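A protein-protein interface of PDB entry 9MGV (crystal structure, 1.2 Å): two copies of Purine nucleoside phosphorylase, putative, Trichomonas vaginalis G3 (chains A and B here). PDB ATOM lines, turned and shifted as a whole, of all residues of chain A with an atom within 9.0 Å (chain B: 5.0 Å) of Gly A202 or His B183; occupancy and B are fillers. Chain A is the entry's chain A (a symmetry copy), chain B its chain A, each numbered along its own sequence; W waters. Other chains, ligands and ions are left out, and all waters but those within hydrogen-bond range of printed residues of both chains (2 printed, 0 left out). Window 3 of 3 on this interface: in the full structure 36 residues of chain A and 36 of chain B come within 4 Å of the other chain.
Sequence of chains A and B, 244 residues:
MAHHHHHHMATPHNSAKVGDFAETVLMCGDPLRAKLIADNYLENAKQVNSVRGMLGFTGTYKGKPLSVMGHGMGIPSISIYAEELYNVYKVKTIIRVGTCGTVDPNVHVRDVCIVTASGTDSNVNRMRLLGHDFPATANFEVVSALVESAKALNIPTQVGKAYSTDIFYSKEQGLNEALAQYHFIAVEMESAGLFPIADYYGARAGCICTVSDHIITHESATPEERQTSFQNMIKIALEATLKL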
ATOM      1  N   TYR A  86      20.070   6.858 -17.172  1.00  0.00           N
ATOM      2  CA  TYR A  86      19.280   6.445 -18.324  1.00  0.00           C
ATOM      3  C   TYR A  86      20.122   5.681 -19.341  1.00  0.00           C
ATOM      4  O   TYR A  86      19.639   4.724 -19.953  1.00  0.00           O
ATOM      5  CB  TYR A  86      18.623   7.647 -18.999  1.00  0.00           C
ATOM      6  CG  TYR A  86      17.494   8.296 -18.230  1.00  0.00           C
ATOM      7  CD1 TYR A  86      16.347   7.584 -17.885  1.00  0.00           C
ATOM      8  CD2 TYR A  86      17.539   9.629 -17.892  1.00  0.00           C
ATOM      9  CE1 TYR A  86      15.307   8.192 -17.202  1.00  0.00           C
ATOM     10  CE2 TYR A  86      16.493  10.242 -17.229  1.00  0.00           C
ATOM     11  CZ  TYR A  86      15.370   9.527 -16.899  1.00  0.00           C
ATOM     12  OH  TYR A  86      14.344  10.176 -16.241  1.00  0.00           O
ATOM     13  N   VAL A  91      17.939   2.889 -16.678  1.00  0.00           N
ATOM     14  CA  VAL A  91      16.786   3.308 -15.896  1.00  0.00           C
ATOM     15  C   VAL A  91      15.682   3.775 -16.824  1.00  0.00           C
ATOM     16  O   VAL A  91      15.934   4.370 -17.878  1.00  0.00           O
ATOM     17  CB  VAL A  91      17.243   4.418 -14.932  1.00  0.00           C
ATOM     18  CG1 VAL A  91      16.088   5.174 -14.297  1.00  0.00           C
ATOM     19  CG2 VAL A  91      18.179   3.820 -13.876  1.00  0.00           C
ATOM     20  N   LYS A  92      14.436   3.532 -16.418  1.00  0.00           N
ATOM     21  CA  LYS A  92      13.262   3.895 -17.200  1.00  0.00           C
ATOM     22  C   LYS A  92      12.509   5.101 -16.650  1.00  0.00           C
ATOM     23  O   LYS A  92      11.909   5.847 -17.435  1.00  0.00           O
ATOM     24  CB  LYS A  92      12.298   2.709 -17.292  1.00  0.00           C
ATOM     25  CG  LYS A  92      12.898   1.450 -17.898  1.00  0.00           C
ATOM     26  CD  LYS A  92      13.337   1.645 -19.334  1.00  0.00           C
ATOM     27  CE  LYS A  92      13.797   0.314 -19.920  1.00  0.00           C
ATOM     28  NZ  LYS A  92      14.178   0.415 -21.347  1.00  0.00           N
ATOM     29  N   THR A  93      12.516   5.301 -15.333  1.00  0.00           N
ATOM     30  CA  THR A  93      11.733   6.351 -14.696  1.00  0.00           C
ATOM     31  C   THR A  93      12.538   6.952 -13.556  1.00  0.00           C
ATOM     32  O   THR A  93      13.013   6.215 -12.687  1.00  0.00           O
ATOM     33  CB  THR A  93      10.427   5.766 -14.115  1.00  0.00           C
ATOM     34  OG1 THR A  93       9.735   5.009 -15.114  1.00  0.00           O
ATOM     35  CG2 THR A  93       9.515   6.857 -13.596  1.00  0.00           C
ATOM     36  N   LEU A 129      17.758  22.260 -28.894  1.00  0.00           N
ATOM     37  CA  LEU A 129      16.685  22.507 -29.853  1.00  0.00           C
ATOM     38  C   LEU A 129      16.977  23.741 -30.699  1.00  0.00           C
ATOM     39  O   LEU A 129      16.132  24.617 -30.898  1.00  0.00           O
ATOM     40  CB  LEU A 129      15.333  22.588 -29.144  1.00  0.00           C
ATOM     41  CG  LEU A 129      14.114  22.420 -30.055  1.00  0.00           C
ATOM     42  CD1 LEU A 129      14.108  21.146 -30.842  1.00  0.00           C
ATOM     43  CD2 LEU A 129      12.828  22.565 -29.253  1.00  0.00           C
ATOM     44  N   PHE A 134      12.499  24.938 -25.632  1.00  0.00           N
ATOM     45  CA  PHE A 134      12.263  23.514 -25.430  1.00  0.00           C
ATOM     46  C   PHE A 134      11.712  23.388 -24.022  1.00  0.00           C
ATOM     47  O   PHE A 134      12.468  23.543 -23.060  1.00  0.00           O
ATOM     48  CB  PHE A 134      13.618  22.813 -25.559  1.00  0.00           C
ATOM     49  CG  PHE A 134      13.626  21.305 -25.357  1.00  0.00           C
ATOM     50  CD1 PHE A 134      12.569  20.587 -24.836  1.00  0.00           C
ATOM     51  CD2 PHE A 134      14.773  20.611 -25.691  1.00  0.00           C
ATOM     52  CE1 PHE A 134      12.673  19.209 -24.646  1.00  0.00           C
ATOM     53  CE2 PHE A 134      14.876  19.256 -25.500  1.00  0.00           C
ATOM     54  CZ  PHE A 134      13.813  18.553 -24.979  1.00  0.00           C
ATOM     55  N   THR A 137       9.495  19.121 -19.659  1.00  0.00           N
ATOM     56  CA  THR A 137       8.120  18.690 -19.421  1.00  0.00           C
ATOM     57  C   THR A 137       8.120  17.323 -18.748  1.00  0.00           C
ATOM     58  O   THR A 137       8.766  16.393 -19.231  1.00  0.00           O
ATOM     59  CB  THR A 137       7.343  18.628 -20.754  1.00  0.00           C
ATOM     60  OG1 THR A 137       7.512  19.861 -21.459  1.00  0.00           O
ATOM     61  CG2 THR A 137       5.880  18.405 -20.521  1.00  0.00           C
ATOM     62  N   ASN A 139       6.677  13.679 -17.668  1.00  0.00           N
ATOM     63  CA  ASN A 139       5.856  12.657 -18.305  1.00  0.00           C
ATOM     64  C   ASN A 139       4.478  12.612 -17.641  1.00  0.00           C
ATOM     65  O   ASN A 139       4.359  12.633 -16.413  1.00  0.00           O
ATOM     66  CB  ASN A 139       6.554  11.312 -18.172  1.00  0.00           C
ATOM     67  CG  ASN A 139       5.679  10.173 -18.601  1.00  0.00           C
ATOM     68  OD1 ASN A 139       4.989   9.565 -17.783  1.00  0.00           O
ATOM     69  ND2 ASN A 139       5.660   9.911 -19.897  1.00  0.00           N
ATOM     70  N   PHE A 195      14.194  16.623 -17.246  1.00  0.00           N
ATOM     71  CA  PHE A 195      13.148  16.195 -18.164  1.00  0.00           C
ATOM     72  C   PHE A 195      13.647  16.034 -19.600  1.00  0.00           C
ATOM     73  O   PHE A 195      13.279  15.036 -20.248  1.00  0.00           O
ATOM     74  CB  PHE A 195      11.955  17.151 -18.069  1.00  0.00           C
ATOM     75  CG  PHE A 195      11.332  17.247 -16.689  1.00  0.00           C
ATOM     76  CD1 PHE A 195      11.407  16.222 -15.741  1.00  0.00           C
ATOM     77  CD2 PHE A 195      10.680  18.401 -16.323  1.00  0.00           C
ATOM     78  CE1 PHE A 195      10.808  16.364 -14.498  1.00  0.00           C
ATOM     79  CE2 PHE A 195      10.084  18.521 -15.088  1.00  0.00           C
ATOM     80  CZ  PHE A 195      10.140  17.501 -14.184  1.00  0.00           C
ATOM     81  N   PRO A 196      14.485  16.923 -20.144  1.00  0.00           N
ATOM     82  CA  PRO A 196      14.948  16.716 -21.532  1.00  0.00           C
ATOM     83  C   PRO A 196      15.860  15.518 -21.691  1.00  0.00           C
ATOM     84  O   PRO A 196      15.907  14.941 -22.784  1.00  0.00           O
ATOM     85  CB  PRO A 196      15.655  18.033 -21.872  1.00  0.00           C
ATOM     86  CG  PRO A 196      14.988  19.049 -20.950  1.00  0.00           C
ATOM     87  CD  PRO A 196      14.813  18.282 -19.664  1.00  0.00           C
ATOM     88  N   ILE A 197      16.612  15.155 -20.648  1.00  0.00           N
ATOM     89  CA  ILE A 197      17.446  13.963 -20.705  1.00  0.00           C
ATOM     90  C   ILE A 197      16.575  12.719 -20.771  1.00  0.00           C
ATOM     91  O   ILE A 197      16.846  11.801 -21.557  1.00  0.00           O
ATOM     92  CB  ILE A 197      18.438  13.931 -19.531  1.00  0.00           C
ATOM     93  CG1 ILE A 197      19.379  15.131 -19.625  1.00  0.00           C
ATOM     94  CG2 ILE A 197      19.206  12.602 -19.508  1.00  0.00           C
ATOM     95  CD1 ILE A 197      20.331  15.239 -18.458  1.00  0.00           C
ATOM     96  N   ALA A 198      15.522  12.659 -19.952  1.00  0.00           N
ATOM     97  CA  ALA A 198      14.572  11.563 -20.085  1.00  0.00           C
ATOM     98  C   ALA A 198      14.057  11.472 -21.517  1.00  0.00           C
ATOM     99  O   ALA A 198      14.002  10.388 -22.100  1.00  0.00           O
ATOM    100  CB  ALA A 198      13.425  11.739 -19.092  1.00  0.00           C
ATOM    101  N   ASP A 199      13.691  12.615 -22.107  1.00  0.00           N
ATOM    102  CA  ASP A 199      13.199  12.622 -23.480  1.00  0.00           C
ATOM    103  C   ASP A 199      14.228  12.021 -24.436  1.00  0.00           C
ATOM    104  O   ASP A 199      13.885  11.211 -25.306  1.00  0.00           O
ATOM    105  CB  ASP A 199      12.895  14.044 -23.948  1.00  0.00           C
ATOM    106  CG  ASP A 199      11.699  14.685 -23.292  1.00  0.00           C
ATOM    107  OD1 ASP A 199      10.826  13.991 -22.744  1.00  0.00           O
ATOM    108  OD2 ASP A 199      11.616  15.936 -23.390  1.00  0.00           O
ATOM    109  N   TYR A 200      15.503  12.411 -24.293  1.00  0.00           N
ATOM    110  CA  TYR A 200      16.537  11.940 -25.210  1.00  0.00           C
ATOM    111  C   TYR A 200      16.575  10.424 -25.246  1.00  0.00           C
ATOM    112  O   TYR A 200      16.819   9.827 -26.300  1.00  0.00           O
ATOM    113  CB  TYR A 200      17.896  12.488 -24.766  1.00  0.00           C
ATOM    114  CG  TYR A 200      19.056  12.113 -25.671  1.00  0.00           C
ATOM    115  CD1 TYR A 200      19.761  10.939 -25.462  1.00  0.00           C
ATOM    116  CD2 TYR A 200      19.430  12.920 -26.728  1.00  0.00           C
ATOM    117  CE1 TYR A 200      20.798  10.571 -26.288  1.00  0.00           C
ATOM    118  CE2 TYR A 200      20.471  12.575 -27.555  1.00  0.00           C
ATOM    119  CZ  TYR A 200      21.155  11.395 -27.336  1.00  0.00           C
ATOM    120  OH  TYR A 200      22.194  11.061 -28.175  1.00  0.00           O
ATOM    121  N   TYR A 201      16.391   9.794 -24.090  1.00  0.00           N
ATOM    122  CA  TYR A 201      16.472   8.347 -23.938  1.00  0.00           C
ATOM    123  C   TYR A 201      15.121   7.663 -24.090  1.00  0.00           C
ATOM    124  O   TYR A 201      15.029   6.455 -23.867  1.00  0.00           O
ATOM    125  CB  TYR A 201      17.151   7.990 -22.598  1.00  0.00           C
ATOM    126  CG  TYR A 201      18.626   8.319 -22.652  1.00  0.00           C
ATOM    127  CD1 TYR A 201      19.479   7.536 -23.386  1.00  0.00           C
ATOM    128  CD2 TYR A 201      19.132   9.456 -22.059  1.00  0.00           C
ATOM    129  CE1 TYR A 201      20.814   7.849 -23.510  1.00  0.00           C
ATOM    130  CE2 TYR A 201      20.467   9.785 -22.161  1.00  0.00           C
ATOM    131  CZ  TYR A 201      21.303   8.977 -22.898  1.00  0.00           C
ATOM    132  OH  TYR A 201      22.636   9.276 -23.065  1.00  0.00           O
ATOM    133  N   GLY A 202      14.075   8.384 -24.491  1.00  0.00           N
ATOM    134  CA  GLY A 202      12.769   7.757 -24.609  1.00  0.00           C
ATOM    135  C   GLY A 202      12.248   7.244 -23.286  1.00  0.00           C
ATOM    136  O   GLY A 202      11.512   6.248 -23.250  1.00  0.00           O
ATOM    137  N   ALA A 203      12.611   7.902 -22.200  1.00  0.00           N
ATOM    138  CA  ALA A 203      12.304   7.480 -20.843  1.00  0.00           C
ATOM    139  C   ALA A 203      11.397   8.514 -20.184  1.00  0.00           C
ATOM    140  O   ALA A 203      10.909   9.441 -20.832  1.00  0.00           O
ATOM    141  CB  ALA A 203      13.611   7.265 -20.074  1.00  0.00           C
ATOM    142  N   ARG A 204      11.182   8.355 -18.879  1.00  0.00           N
ATOM    143  CA  ARG A 204      10.188   9.122 -18.146  1.00  0.00           C
ATOM    144  C   ARG A 204      10.802   9.810 -16.941  1.00  0.00           C
ATOM    145  O   ARG A 204      11.674   9.245 -16.274  1.00  0.00           O
ATOM    146  CB  ARG A 204       9.083   8.172 -17.605  1.00  0.00           C
ATOM    147  CG  ARG A 204       8.252   7.545 -18.695  1.00  0.00           C
ATOM    148  CD  ARG A 204       7.259   6.591 -18.110  1.00  0.00           C
ATOM    149  NE  ARG A 204       6.149   6.347 -19.030  1.00  0.00           N
ATOM    150  CZ  ARG A 204       5.044   5.702 -18.686  1.00  0.00           C
ATOM    151  NH1 ARG A 204       4.896   5.209 -17.478  1.00  0.00           N
ATOM    152  NH2 ARG A 204       4.051   5.575 -19.566  1.00  0.00           N
ATOM    153  N   ALA A 205      10.270  10.991 -16.622  1.00  0.00           N
ATOM    154  CA  ALA A 205      10.674  11.700 -15.423  1.00  0.00           C
ATOM    155  C   ALA A 205       9.529  12.541 -14.885  1.00  0.00           C
ATOM    156  O   ALA A 205       8.607  12.914 -15.606  1.00  0.00           O
ATOM    157  CB  ALA A 205      11.889  12.595 -15.672  1.00  0.00           C
ATOM    158  N   ASP B 104       7.629  12.185 -35.252  1.00  0.00           N
ATOM    159  CA  ASP B 104       7.977  11.090 -34.357  1.00  0.00           C
ATOM    160  C   ASP B 104       7.687   9.769 -35.060  1.00  0.00           C
ATOM    161  O   ASP B 104       6.590   9.585 -35.592  1.00  0.00           O
ATOM    162  CB  ASP B 104       7.161  11.200 -33.070  1.00  0.00           C
ATOM    163  CG  ASP B 104       7.639  10.240 -31.989  1.00  0.00           C
ATOM    164  OD1 ASP B 104       8.204  10.708 -30.981  1.00  0.00           O
ATOM    165  OD2 ASP B 104       7.469   9.014 -32.154  1.00  0.00           O
ATOM    166  N   LYS B 161       4.620  16.441 -25.848  1.00  0.00           N
ATOM    167  CA  LYS B 161       4.971  17.803 -26.220  1.00  0.00           C
ATOM    168  C   LYS B 161       4.599  18.138 -27.661  1.00  0.00           C
ATOM    169  O   LYS B 161       4.794  17.339 -28.572  1.00  0.00           O
ATOM    170  CB  LYS B 161       6.478  18.012 -26.087  1.00  0.00           C
ATOM    171  CG  LYS B 161       7.056  17.862 -24.690  1.00  0.00           C
ATOM    172  CD  LYS B 161       8.556  18.114 -24.662  1.00  0.00           C
ATOM    173  CE  LYS B 161       9.364  17.198 -25.569  1.00  0.00           C
ATOM    174  NZ  LYS B 161       9.261  15.783 -25.165  1.00  0.00           N
ATOM    175  N   LEU B 179      13.520  17.606 -33.114  1.00  0.00           N
ATOM    176  CA  LEU B 179      12.167  17.348 -32.630  1.00  0.00           C
ATOM    177  C   LEU B 179      11.941  15.858 -32.415  1.00  0.00           C
ATOM    178  O   LEU B 179      11.334  15.452 -31.420  1.00  0.00           O
ATOM    179  CB  LEU B 179      11.150  17.911 -33.621  1.00  0.00           C
ATOM    180  CG  LEU B 179      11.088  19.428 -33.738  1.00  0.00           C
ATOM    181  CD1 LEU B 179      10.172  19.865 -34.871  1.00  0.00           C
ATOM    182  CD2 LEU B 179      10.617  20.075 -32.433  1.00  0.00           C
ATOM    183  N   ALA B 180      12.440  15.028 -33.330  1.00  0.00           N
ATOM    184  CA  ALA B 180      12.285  13.584 -33.191  1.00  0.00           C
ATOM    185  C   ALA B 180      13.137  13.038 -32.048  1.00  0.00           C
ATOM    186  O   ALA B 180      12.685  12.173 -31.287  1.00  0.00           O
ATOM    187  CB  ALA B 180      12.631  12.903 -34.518  1.00  0.00           C
ATOM    188  N   GLN B 181      14.371  13.538 -31.908  1.00  0.00           N
ATOM    189  CA  GLN B 181      15.266  13.060 -30.857  1.00  0.00           C
ATOM    190  C   GLN B 181      14.645  13.213 -29.477  1.00  0.00           C
ATOM    191  O   GLN B 181      14.878  12.391 -28.586  1.00  0.00           O
ATOM    192  CB  GLN B 181      16.589  13.836 -30.919  1.00  0.00           C
ATOM    193  CG  GLN B 181      17.586  13.460 -29.837  1.00  0.00           C
ATOM    194  CD  GLN B 181      18.185  12.120 -30.101  1.00  0.00           C
ATOM    195  OE1 GLN B 181      19.041  11.985 -30.973  1.00  0.00           O
ATOM    196  NE2 GLN B 181      17.755  11.106 -29.349  1.00  0.00           N
ATOM    197  N   TYR B 182      13.889  14.281 -29.270  1.00  0.00           N
ATOM    198  CA  TYR B 182      13.309  14.601 -27.970  1.00  0.00           C
ATOM    199  C   TYR B 182      11.815  14.285 -27.907  1.00  0.00           C
ATOM    200  O   TYR B 182      11.140  14.658 -26.939  1.00  0.00           O
ATOM    201  CB  TYR B 182      13.641  16.052 -27.586  1.00  0.00           C
ATOM    202  CG  TYR B 182      15.134  16.202 -27.335  1.00  0.00           C
ATOM    203  CD1 TYR B 182      15.682  15.835 -26.106  1.00  0.00           C
ATOM    204  CD2 TYR B 182      16.005  16.651 -28.332  1.00  0.00           C
ATOM    205  CE1 TYR B 182      17.048  15.938 -25.873  1.00  0.00           C
ATOM    206  CE2 TYR B 182      17.381  16.746 -28.090  1.00  0.00           C
ATOM    207  CZ  TYR B 182      17.884  16.373 -26.872  1.00  0.00           C
ATOM    208  OH  TYR B 182      19.229  16.442 -26.612  1.00  0.00           O
ATOM    209  N   HIS B 183      11.297  13.575 -28.909  1.00  0.00           N
ATOM    210  CA  HIS B 183       9.944  13.026 -28.878  1.00  0.00           C
ATOM    211  C   HIS B 183       8.882  14.111 -28.754  1.00  0.00           C
ATOM    212  O   HIS B 183       7.897  13.960 -28.039  1.00  0.00           O
ATOM    213  CB  HIS B 183       9.808  11.946 -27.816  1.00  0.00           C
ATOM    214  CG  HIS B 183      10.687  10.778 -28.078  1.00  0.00           C
ATOM    215  ND1 HIS B 183      10.372   9.825 -29.020  1.00  0.00           N
ATOM    216  CD2 HIS B 183      11.891  10.424 -27.569  1.00  0.00           C
ATOM    217  CE1 HIS B 183      11.332   8.917 -29.057  1.00  0.00           C
ATOM    218  NE2 HIS B 183      12.265   9.258 -28.186  1.00  0.00           N
ATOM    219  N   PHE B 184       9.042  15.182 -29.526  1.00  0.00           N
ATOM    220  CA  PHE B 184       7.931  16.082 -29.783  1.00  0.00           C
ATOM    221  C   PHE B 184       6.947  15.355 -30.680  1.00  0.00           C
ATOM    222  O   PHE B 184       7.325  14.865 -31.750  1.00  0.00           O
ATOM    223  CB  PHE B 184       8.428  17.363 -30.452  1.00  0.00           C
ATOM    224  CG  PHE B 184       9.135  18.293 -29.513  1.00  0.00           C
ATOM    225  CD1 PHE B 184      10.476  18.114 -29.176  1.00  0.00           C
ATOM    226  CD2 PHE B 184       8.448  19.349 -28.939  1.00  0.00           C
ATOM    227  CE1 PHE B 184      11.103  18.969 -28.294  1.00  0.00           C
ATOM    228  CE2 PHE B 184       9.079  20.212 -28.066  1.00  0.00           C
ATOM    229  CZ  PHE B 184      10.403  20.017 -27.743  1.00  0.00           C
ATOM    230  N   ILE B 185       5.683  15.297 -30.256  1.00  0.00           N
ATOM    231  CA  ILE B 185       4.696  14.477 -30.960  1.00  0.00           C
ATOM    232  C   ILE B 185       3.887  15.249 -31.993  1.00  0.00           C
ATOM    233  O   ILE B 185       3.341  14.627 -32.913  1.00  0.00           O
ATOM    234  CB  ILE B 185       3.770  13.709 -29.992  1.00  0.00           C
ATOM    235  CG1 ILE B 185       2.887  14.654 -29.171  1.00  0.00           C
ATOM    236  CG2 ILE B 185       4.591  12.809 -29.073  1.00  0.00           C
ATOM    237  CD1 ILE B 185       1.800  13.944 -28.349  1.00  0.00           C
HETATM  238  O   HOH W   1      15.003   8.980 -28.172  1.00  0.00           O
HETATM  239  O   HOH W   2       8.769  15.486 -21.902  1.00  0.00           O
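Hydrophobic or aromatic side chains of chain A that line the printed part of chain B: Leu A129, Phe A134 and Tyr A200.
Of the 9 printed residues of chain B, 6 touch a printed residue of chain A.
Among the printed residues, Asp or Glu carboxylates within 4 Å of a Lys or Arg side-chain nitrogen of the other chain: Asp A199 with Lys B161.
Water W2 lies within hydrogen-bond range of OD1 of Asp A199 (2.7 Å), O of Thr A137 (2.8 Å) and NZ of Lys B161 (3.3 Å).
Water W1 lies within hydrogen-bond range of the backbone carbonyl oxygen of Tyr A200 (2.7 Å), a ring nitrogen (NE2) of His B183 (2.8 Å) and the backbone carbonyl oxygen of Gln B181 (3.4 Å).
Gly A202 touches just one residue of chain B: His B183 (3.9 Å).
His B183 touches just these residues of chain A: Asp A199 (3.1 Å) and Gly A202 (3.9 Å).
Printed residues of chain A within 4 Å of Leu B179: Leu A129 (3.98 Å).
Printed residues of chain B within 4 Å of Leu A129: Leu B179 and Phe B184.
Of the printed residues of chain B, Pro A196 touches Tyr B182.
Printed residues of chain B within 4 Å of Tyr A200: Gln B181 (3.4 Å) and Tyr B182 (3.5 Å).
Thr A93 touches none of the printed residues of chain B.
The nearest printed residue of chain B that does not touch Phe A134 is His B183 (6.8 Å).
CD1 of Leu A129 touches CD2 of Leu B179 (3.98 Å).
Leu A129 touches Phe B184 (CD2 to CZ, 3.8 Å).
Phe A134 touches Lys B161.
Phe A134 touches Tyr B182.
Phe A134 touches Phe B184.
CD of Lys B161 touches OG1 of Thr A137 (3.8 Å).
Asp A199 touches Gln B181 (O to O, 3.6 Å).
Asp A199 touches His B183.
Tyr A200 touches Tyr B182 (CD2 to OH, 3.5 Å).
His B183 touches Gly A202.
NZ of Lys B161 is in salt-bridge range of OD2 of Asp A199 (3.0 Å).
The backbone carbonyl oxygen (O) of Tyr A200 lies within hydrogen-bond range of the side-chain amide nitrogen (NE2) of Gln B181, 3.4 Å away.
OD1 of Asp B104 lies within hydrogen-bond range of ND1 of His B183 (3.1 Å).
The side-chain amino group (NZ) of Lys B161 sits at hydrogen-bond distance from the backbone carbonyl oxygen (O) of Tyr B182 (2.8 Å).
The backbone carbonyl oxygen (O) of Leu B179 is in hydrogen-bond range of the backbone NH (N) of Phe B184, 3.0 Å away.
O of Lys B161 lies within hydrogen-bond range of N of Ile B185, 2.8 Å away.
No position is printed for both chains.
Of the 14 pairs that touch across the chains among the printed residues, none has its exchanged pair printed and touching as well.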
